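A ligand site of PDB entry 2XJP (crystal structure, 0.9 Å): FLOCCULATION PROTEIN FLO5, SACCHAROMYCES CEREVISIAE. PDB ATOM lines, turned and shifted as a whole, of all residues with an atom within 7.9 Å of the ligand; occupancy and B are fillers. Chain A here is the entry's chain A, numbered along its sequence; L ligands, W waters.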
ATOM      1  N   ILE A  28      -3.611  13.671 -10.390  1.00  0.00           N
ATOM      2  CA  ILE A  28      -3.326  15.071 -10.082  1.00  0.00           C
ATOM      3  C   ILE A  28      -3.171  15.197  -8.589  1.00  0.00           C
ATOM      4  O   ILE A  28      -4.095  14.945  -7.827  1.00  0.00           O
ATOM      5  CB  ILE A  28      -4.434  16.036 -10.546  1.00  0.00           C
ATOM      6  CG1 ILE A  28      -5.050  15.706 -11.876  1.00  0.00           C
ATOM      7  CG2 ILE A  28      -3.932  17.469 -10.415  1.00  0.00           C
ATOM      8  CD1 ILE A  28      -4.116  15.836 -12.941  1.00  0.00           C
ATOM      9  N   PHE A  30      -2.171  17.947  -5.507  1.00  0.00           N
ATOM     10  CA  PHE A  30      -2.241  19.362  -5.231  1.00  0.00           C
ATOM     11  C   PHE A  30      -1.412  19.687  -4.004  1.00  0.00           C
ATOM     12  O   PHE A  30      -1.465  18.962  -3.008  1.00  0.00           O
ATOM     13  CB  PHE A  30      -3.701  19.781  -4.926  1.00  0.00           C
ATOM     14  CG  PHE A  30      -4.628  19.593  -6.069  1.00  0.00           C
ATOM     15  CD1 PHE A  30      -4.958  20.653  -6.899  1.00  0.00           C
ATOM     16  CD2 PHE A  30      -5.202  18.356  -6.368  1.00  0.00           C
ATOM     17  CE1 PHE A  30      -5.842  20.508  -7.934  1.00  0.00           C
ATOM     18  CE2 PHE A  30      -6.078  18.181  -7.414  1.00  0.00           C
ATOM     19  CZ  PHE A  30      -6.417  19.278  -8.190  1.00  0.00           C
ATOM     20  N   VAL A  60      -6.668  13.867  -7.080  1.00  0.00           N
ATOM     21  CA  VAL A  60      -7.720  13.208  -7.817  1.00  0.00           C
ATOM     22  C   VAL A  60      -7.068  12.379  -8.926  1.00  0.00           C
ATOM     23  O   VAL A  60      -6.069  12.730  -9.472  1.00  0.00           O
ATOM     24  CB  VAL A  60      -8.707  14.206  -8.474  1.00  0.00           C
ATOM     25  CG1 VAL A  60      -9.369  15.186  -7.531  1.00  0.00           C
ATOM     26  CG2 VAL A  60      -8.025  15.056  -9.478  1.00  0.00           C
ATOM     27  N   GLN A  63      -7.832  11.551 -14.618  1.00  0.00           N
ATOM     28  CA  GLN A  63      -8.166  12.764 -15.350  1.00  0.00           C
ATOM     29  C   GLN A  63      -7.611  12.730 -16.767  1.00  0.00           C
ATOM     30  O   GLN A  63      -6.401  12.608 -16.963  1.00  0.00           O
ATOM     31  CB  GLN A  63      -7.610  13.994 -14.613  1.00  0.00           C
ATOM     32  CG  GLN A  63      -8.188  14.105 -13.198  1.00  0.00           C
ATOM     33  CD  GLN A  63      -9.680  14.223 -13.176  1.00  0.00           C
ATOM     34  OE1 GLN A  63     -10.210  15.175 -13.760  1.00  0.00           O
ATOM     35  NE2 GLN A  63     -10.366  13.312 -12.527  1.00  0.00           N
ATOM     36  N   THR A  64      -8.502  12.867 -17.750  1.00  0.00           N
ATOM     37  CA  THR A  64      -8.096  12.871 -19.143  1.00  0.00           C
ATOM     38  C   THR A  64      -8.138  14.254 -19.784  1.00  0.00           C
ATOM     39  O   THR A  64      -7.442  14.493 -20.752  1.00  0.00           O
ATOM     40  CB  THR A  64      -8.931  11.897 -19.956  1.00  0.00           C
ATOM     41  OG1 THR A  64     -10.311  12.193 -19.771  1.00  0.00           O
ATOM     42  CG2 THR A  64      -8.666  10.478 -19.568  1.00  0.00           C
ATOM     43  N   ASP A  65      -8.940  15.156 -19.215  1.00  0.00           N
ATOM     44  CA  ASP A  65      -9.036  16.536 -19.682  1.00  0.00           C
ATOM     45  C   ASP A  65      -8.142  17.353 -18.757  1.00  0.00           C
ATOM     46  O   ASP A  65      -8.450  17.458 -17.559  1.00  0.00           O
ATOM     47  CB  ASP A  65     -10.478  17.009 -19.619  1.00  0.00           C
ATOM     48  CG  ASP A  65     -11.411  16.235 -20.529  1.00  0.00           C
ATOM     49  OD1 ASP A  65     -11.320  16.415 -21.748  1.00  0.00           O
ATOM     50  OD2 ASP A  65     -12.271  15.478 -20.055  1.00  0.00           O
ATOM     51  N   ILE A  66      -7.009  17.818 -19.279  1.00  0.00           N
ATOM     52  CA  ILE A  66      -5.912  18.278 -18.457  1.00  0.00           C
ATOM     53  C   ILE A  66      -5.533  19.736 -18.605  1.00  0.00           C
ATOM     54  O   ILE A  66      -4.674  20.222 -17.884  1.00  0.00           O
ATOM     55  CB  ILE A  66      -4.654  17.382 -18.617  1.00  0.00           C
ATOM     56  CG1 ILE A  66      -4.122  17.360 -20.046  1.00  0.00           C
ATOM     57  CG2 ILE A  66      -4.978  15.984 -18.013  1.00  0.00           C
ATOM     58  CD1 ILE A  66      -2.743  16.711 -20.232  1.00  0.00           C
ATOM     59  N   SER A  67      -6.158  20.483 -19.514  1.00  0.00           N
ATOM     60  CA  SER A  67      -5.845  21.905 -19.597  1.00  0.00           C
ATOM     61  C   SER A  67      -6.454  22.667 -18.434  1.00  0.00           C
ATOM     62  O   SER A  67      -7.474  22.292 -17.850  1.00  0.00           O
ATOM     63  CB  SER A  67      -6.367  22.484 -20.900  1.00  0.00           C
ATOM     64  OG  SER A  67      -5.548  21.990 -21.959  1.00  0.00           O
ATOM     65  N   ILE A  68      -5.824  23.794 -18.127  1.00  0.00           N
ATOM     66  CA  ILE A  68      -6.320  24.658 -17.043  1.00  0.00           C
ATOM     67  C   ILE A  68      -6.760  25.974 -17.639  1.00  0.00           C
ATOM     68  O   ILE A  68      -6.082  26.597 -18.454  1.00  0.00           O
ATOM     69  CB  ILE A  68      -5.230  24.847 -16.000  1.00  0.00           C
ATOM     70  CG1 ILE A  68      -4.964  23.469 -15.408  1.00  0.00           C
ATOM     71  CG2 ILE A  68      -5.654  25.884 -14.897  1.00  0.00           C
ATOM     72  CD1 ILE A  68      -3.690  23.474 -14.627  1.00  0.00           C
ATOM     73  N   ASP A  69      -7.924  26.385 -17.198  1.00  0.00           N
ATOM     74  CA  ASP A  69      -8.504  27.689 -17.593  1.00  0.00           C
ATOM     75  C   ASP A  69      -9.355  28.175 -16.446  1.00  0.00           C
ATOM     76  O   ASP A  69     -10.572  28.010 -16.416  1.00  0.00           O
ATOM     77  CB  ASP A  69      -9.342  27.590 -18.881  1.00  0.00           C
ATOM     78  CG  ASP A  69      -9.879  28.913 -19.312  1.00  0.00           C
ATOM     79  OD1 ASP A  69      -9.456  29.948 -18.834  1.00  0.00           O
ATOM     80  OD2 ASP A  69     -10.786  28.893 -20.152  1.00  0.00           O
ATOM     81  N   TYR A  70      -8.712  28.746 -15.438  1.00  0.00           N
ATOM     82  CA  TYR A  70      -9.341  29.202 -14.214  1.00  0.00           C
ATOM     83  C   TYR A  70      -9.523  30.735 -14.302  1.00  0.00           C
ATOM     84  O   TYR A  70      -8.572  31.473 -14.498  1.00  0.00           O
ATOM     85  CB  TYR A  70      -8.483  28.862 -12.982  1.00  0.00           C
ATOM     86  CG  TYR A  70      -9.034  29.524 -11.754  1.00  0.00           C
ATOM     87  CD1 TYR A  70     -10.265  29.174 -11.239  1.00  0.00           C
ATOM     88  CD2 TYR A  70      -8.360  30.603 -11.153  1.00  0.00           C
ATOM     89  CE1 TYR A  70     -10.826  29.848 -10.151  1.00  0.00           C
ATOM     90  CE2 TYR A  70      -8.897  31.281 -10.093  1.00  0.00           C
ATOM     91  CZ  TYR A  70     -10.130  30.906  -9.595  1.00  0.00           C
ATOM     92  OH  TYR A  70     -10.659  31.635  -8.538  1.00  0.00           O
ATOM     93  N   THR A 111     -13.953  24.335  -7.300  1.00  0.00           N
ATOM     94  CA  THR A 111     -13.641  23.009  -7.821  1.00  0.00           C
ATOM     95  C   THR A 111     -13.179  23.020  -9.285  1.00  0.00           C
ATOM     96  O   THR A 111     -13.090  21.957  -9.903  1.00  0.00           O
ATOM     97  CB  THR A 111     -14.880  22.111  -7.696  1.00  0.00           C
ATOM     98  OG1 THR A 111     -15.952  22.747  -8.416  1.00  0.00           O
ATOM     99  CG2 THR A 111     -15.237  21.801  -6.258  1.00  0.00           C
ATOM    100  N   ASP A 112     -12.879  24.189  -9.834  1.00  0.00           N
ATOM    101  CA  ASP A 112     -12.489  24.312 -11.239  1.00  0.00           C
ATOM    102  C   ASP A 112     -11.345  23.373 -11.653  1.00  0.00           C
ATOM    103  O   ASP A 112     -11.313  22.931 -12.790  1.00  0.00           O
ATOM    104  CB  ASP A 112     -12.088  25.755 -11.528  1.00  0.00           C
ATOM    105  CG  ASP A 112     -11.976  26.019 -13.017  1.00  0.00           C
ATOM    106  OD1 ASP A 112     -10.827  26.249 -13.448  1.00  0.00           O
ATOM    107  OD2 ASP A 112     -13.012  25.865 -13.711  1.00  0.00           O
ATOM    108  N   LEU A 113     -10.391  23.160 -10.765  1.00  0.00           N
ATOM    109  CA  LEU A 113      -9.248  22.296 -11.075  1.00  0.00           C
ATOM    110  C   LEU A 113      -9.632  20.867 -10.754  1.00  0.00           C
ATOM    111  O   LEU A 113      -9.490  20.384  -9.632  1.00  0.00           O
ATOM    112  CB  LEU A 113      -8.024  22.730 -10.326  1.00  0.00           C
ATOM    113  CG  LEU A 113      -7.599  24.201 -10.501  1.00  0.00           C
ATOM    114  CD1 LEU A 113      -6.412  24.506  -9.610  1.00  0.00           C
ATOM    115  CD2 LEU A 113      -7.313  24.551 -11.932  1.00  0.00           C
ATOM    116  N   PHE A 114     -10.124  20.135 -11.750  1.00  0.00           N
ATOM    117  CA  PHE A 114     -10.279  18.662 -11.653  1.00  0.00           C
ATOM    118  C   PHE A 114     -11.364  18.214 -10.667  1.00  0.00           C
ATOM    119  O   PHE A 114     -11.400  17.050 -10.314  1.00  0.00           O
ATOM    120  CB  PHE A 114      -8.932  17.952 -11.425  1.00  0.00           C
ATOM    121  CG  PHE A 114      -7.903  18.310 -12.449  1.00  0.00           C
ATOM    122  CD1 PHE A 114      -7.948  17.732 -13.677  1.00  0.00           C
ATOM    123  CD2 PHE A 114      -6.919  19.251 -12.183  1.00  0.00           C
ATOM    124  CE1 PHE A 114      -6.999  18.007 -14.654  1.00  0.00           C
ATOM    125  CE2 PHE A 114      -6.021  19.597 -13.147  1.00  0.00           C
ATOM    126  CZ  PHE A 114      -6.038  18.959 -14.400  1.00  0.00           C
ATOM    127  N   GLY A 115     -12.265  19.115 -10.275  1.00  0.00           N
ATOM    128  CA  GLY A 115     -13.286  18.791  -9.304  1.00  0.00           C
ATOM    129  C   GLY A 115     -12.812  18.851  -7.858  1.00  0.00           C
ATOM    130  O   GLY A 115     -13.614  18.609  -6.955  1.00  0.00           O
ATOM    131  N   PHE A 116     -11.543  19.172  -7.626  1.00  0.00           N
ATOM    132  CA  PHE A 116     -10.975  19.164  -6.276  1.00  0.00           C
ATOM    133  C   PHE A 116     -11.139  20.564  -5.676  1.00  0.00           C
ATOM    134  O   PHE A 116     -10.693  21.545  -6.243  1.00  0.00           O
ATOM    135  CB  PHE A 116      -9.467  18.823  -6.348  1.00  0.00           C
ATOM    136  CG  PHE A 116      -8.821  18.773  -5.021  1.00  0.00           C
ATOM    137  CD1 PHE A 116      -9.067  17.733  -4.155  1.00  0.00           C
ATOM    138  CD2 PHE A 116      -7.929  19.754  -4.655  1.00  0.00           C
ATOM    139  CE1 PHE A 116      -8.489  17.703  -2.898  1.00  0.00           C
ATOM    140  CE2 PHE A 116      -7.307  19.750  -3.427  1.00  0.00           C
ATOM    141  CZ  PHE A 116      -7.616  18.728  -2.521  1.00  0.00           C
ATOM    142  N   LEU A 125       0.262  22.054  -8.762  1.00  0.00           N
ATOM    143  CA  LEU A 125      -0.299  20.742  -8.917  1.00  0.00           C
ATOM    144  C   LEU A 125       0.608  20.011  -9.877  1.00  0.00           C
ATOM    145  O   LEU A 125       1.243  20.585 -10.755  1.00  0.00           O
ATOM    146  CB  LEU A 125      -1.747  20.782  -9.412  1.00  0.00           C
ATOM    147  CG  LEU A 125      -2.005  21.515 -10.755  1.00  0.00           C
ATOM    148  CD1 LEU A 125      -1.760  20.584 -11.965  1.00  0.00           C
ATOM    149  CD2 LEU A 125      -3.420  22.079 -10.795  1.00  0.00           C
ATOM    150  N   MET A 127       0.663  16.675 -12.361  1.00  0.00           N
ATOM    151  CA  MET A 127      -0.053  15.691 -13.146  1.00  0.00           C
ATOM    152  C   MET A 127       0.962  14.609 -13.507  1.00  0.00           C
ATOM    153  O   MET A 127       2.027  14.917 -14.037  1.00  0.00           O
ATOM    154  CB  MET A 127      -0.605  16.298 -14.448  1.00  0.00           C
ATOM    155  CG  MET A 127      -1.219  17.668 -14.276  1.00  0.00           C
ATOM    156  SD  MET A 127      -2.009  18.143 -15.841  1.00  0.00           S
ATOM    157  CE  MET A 127      -2.346  19.871 -15.528  1.00  0.00           C
ATOM    158  N   GLY A 216      -5.578  31.595 -13.837  1.00  0.00           N
ATOM    159  CA  GLY A 216      -4.651  30.497 -14.088  1.00  0.00           C
ATOM    160  C   GLY A 216      -4.921  29.910 -15.458  1.00  0.00           C
ATOM    161  O   GLY A 216      -6.079  29.652 -15.784  1.00  0.00           O
ATOM    162  N   LEU A 218      -3.305  27.156 -18.606  1.00  0.00           N
ATOM    163  CA  LEU A 218      -2.302  26.223 -19.145  1.00  0.00           C
ATOM    164  C   LEU A 218      -3.016  25.346 -20.192  1.00  0.00           C
ATOM    165  O   LEU A 218      -3.565  24.286 -19.882  1.00  0.00           O
ATOM    166  CB  LEU A 218      -1.698  25.337 -18.068  1.00  0.00           C
ATOM    167  CG  LEU A 218      -0.454  24.585 -18.559  1.00  0.00           C
ATOM    168  CD1 LEU A 218       0.736  25.516 -18.811  1.00  0.00           C
ATOM    169  CD2 LEU A 218      -0.072  23.510 -17.540  1.00  0.00           C
ATOM    170  N   ASP A 232      -6.247  19.504 -25.034  1.00  0.00           N
ATOM    171  CA  ASP A 232      -7.048  19.562 -23.805  1.00  0.00           C
ATOM    172  C   ASP A 232      -7.535  18.202 -23.335  1.00  0.00           C
ATOM    173  O   ASP A 232      -7.231  17.787 -22.215  1.00  0.00           O
ATOM    174  CB  ASP A 232      -8.187  20.590 -23.929  1.00  0.00           C
ATOM    175  CG  ASP A 232      -7.754  21.926 -24.603  1.00  0.00           C
ATOM    176  OD1 ASP A 232      -6.831  22.669 -24.125  1.00  0.00           O
ATOM    177  OD2 ASP A 232      -8.404  22.293 -25.627  1.00  0.00           O
ATOM    178  N   ASN A 233      -8.210  17.461 -24.232  1.00  0.00           N
ATOM    179  CA  ASN A 233      -8.764  16.133 -23.975  1.00  0.00           C
ATOM    180  C   ASN A 233      -7.790  15.110 -24.522  1.00  0.00           C
ATOM    181  O   ASN A 233      -7.619  14.928 -25.743  1.00  0.00           O
ATOM    182  CB  ASN A 233     -10.145  15.981 -24.611  1.00  0.00           C
ATOM    183  CG  ASN A 233     -10.707  14.593 -24.495  1.00  0.00           C
ATOM    184  OD1 ASN A 233     -10.182  13.742 -23.774  1.00  0.00           O
ATOM    185  ND2 ASN A 233     -11.873  14.405 -25.081  1.00  0.00           N
HETATM  186  C1  LIG L   1     -11.761  19.225 -14.807  1.00  0.00           C
HETATM  187  C2  LIG L   1     -12.546  19.527 -16.084  1.00  0.00           C
HETATM  188  C3  LIG L   1     -11.547  19.618 -17.229  1.00  0.00           C
HETATM  189  C4  LIG L   1     -10.425  20.602 -16.889  1.00  0.00           C
HETATM  190  C5  LIG L   1      -9.810  20.221 -15.554  1.00  0.00           C
HETATM  191  C6  LIG L   1      -8.735  21.143 -15.010  1.00  0.00           C
HETATM  192  O1  LIG L   1     -12.668  19.154 -13.707  1.00  0.00           O
HETATM  193  O2  LIG L   1     -13.269  20.731 -15.917  1.00  0.00           O
HETATM  194  O3  LIG L   1     -12.245  20.048 -18.372  1.00  0.00           O
HETATM  195  O4  LIG L   1      -9.474  20.482 -17.949  1.00  0.00           O
HETATM  196  O5  LIG L   1     -10.804  20.277 -14.555  1.00  0.00           O
HETATM  197  O6  LIG L   1      -9.126  22.452 -14.859  1.00  0.00           O
HETATM  198  O   HOH W   1     -14.131  21.031 -12.472  1.00  0.00           O
HETATM  199  O   HOH W   2     -12.549  16.598 -13.609  1.00  0.00           O
HETATM  200  O   HOH W   3      -9.443  25.007 -15.348  1.00  0.00           O
HETATM  201  O   HOH W   4     -12.884  23.121 -14.975  1.00  0.00           O
HETATM  202  O   HOH W   5     -12.847  22.486 -18.728  1.00  0.00           O
HETATM  203  O   HOH W   6      -9.194  20.313 -20.612  1.00  0.00           O
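The backbone NH (N) of Ile 66 lies within hydrogen-bond range of the backbone carbonyl oxygen (O) of Asp 232. OD1 of Asp 232 sits at hydrogen-bond distance from OG of Ser 67.
Water W2 bridges an oxygen (O1) of the ligand (2.6 Å) and the side-chain amide oxygen (OE1) of Gln 63 (2.7 Å). Water W4 bridges O2 of the ligand (2.6 Å) and O of Asp 112 (2.7 Å). Water W3 lies within hydrogen-bond range of an oxygen (O6) of the ligand, the side-chain carboxylate of Asp 112 and the backbone NH of Asp 69. Water W1 lies within hydrogen-bond range of O1 of the ligand (2.7 Å), O of Thr 111 (2.9 Å), O of Asp 112 (3.4 Å) and N of Gly 115 (3.5 Å). Water W6 lies within hydrogen-bond range of an oxygen (O4) of the ligand and the backbone NH (N) of Ser 67.
Residues that only touch the ligand: Leu 113 and Ile 66. Hydrophobic or aromatic side chains within 4 Å of the ligand: Phe 114. Within 4 Å of the ligand: Asp 65, Ile 66, Ser 67, Asp 112, Leu 113, Phe 114 and Gly 115. The nearest printed residue that does not touch the ligand is Ile 68 (4.2 Å).
N of Phe 114 sits at hydrogen-bond distance from O5 of the ligand. O1 of the ligand sits at hydrogen-bond distance from N of Gly 115 (3.5 Å). The backbone carbonyl oxygen (O) of Ser 67 lies within hydrogen-bond range of an oxygen (O4) of the ligand, 2.7 Å away. The backbone carbonyl oxygen of Asp 65 is in hydrogen-bond range of an oxygen (O4) of the ligand, 3.2 Å away. The backbone carbonyl oxygen (O) of Asp 112 sits at hydrogen-bond distance from an oxygen (O6) of the ligand, 3.0 Å away.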
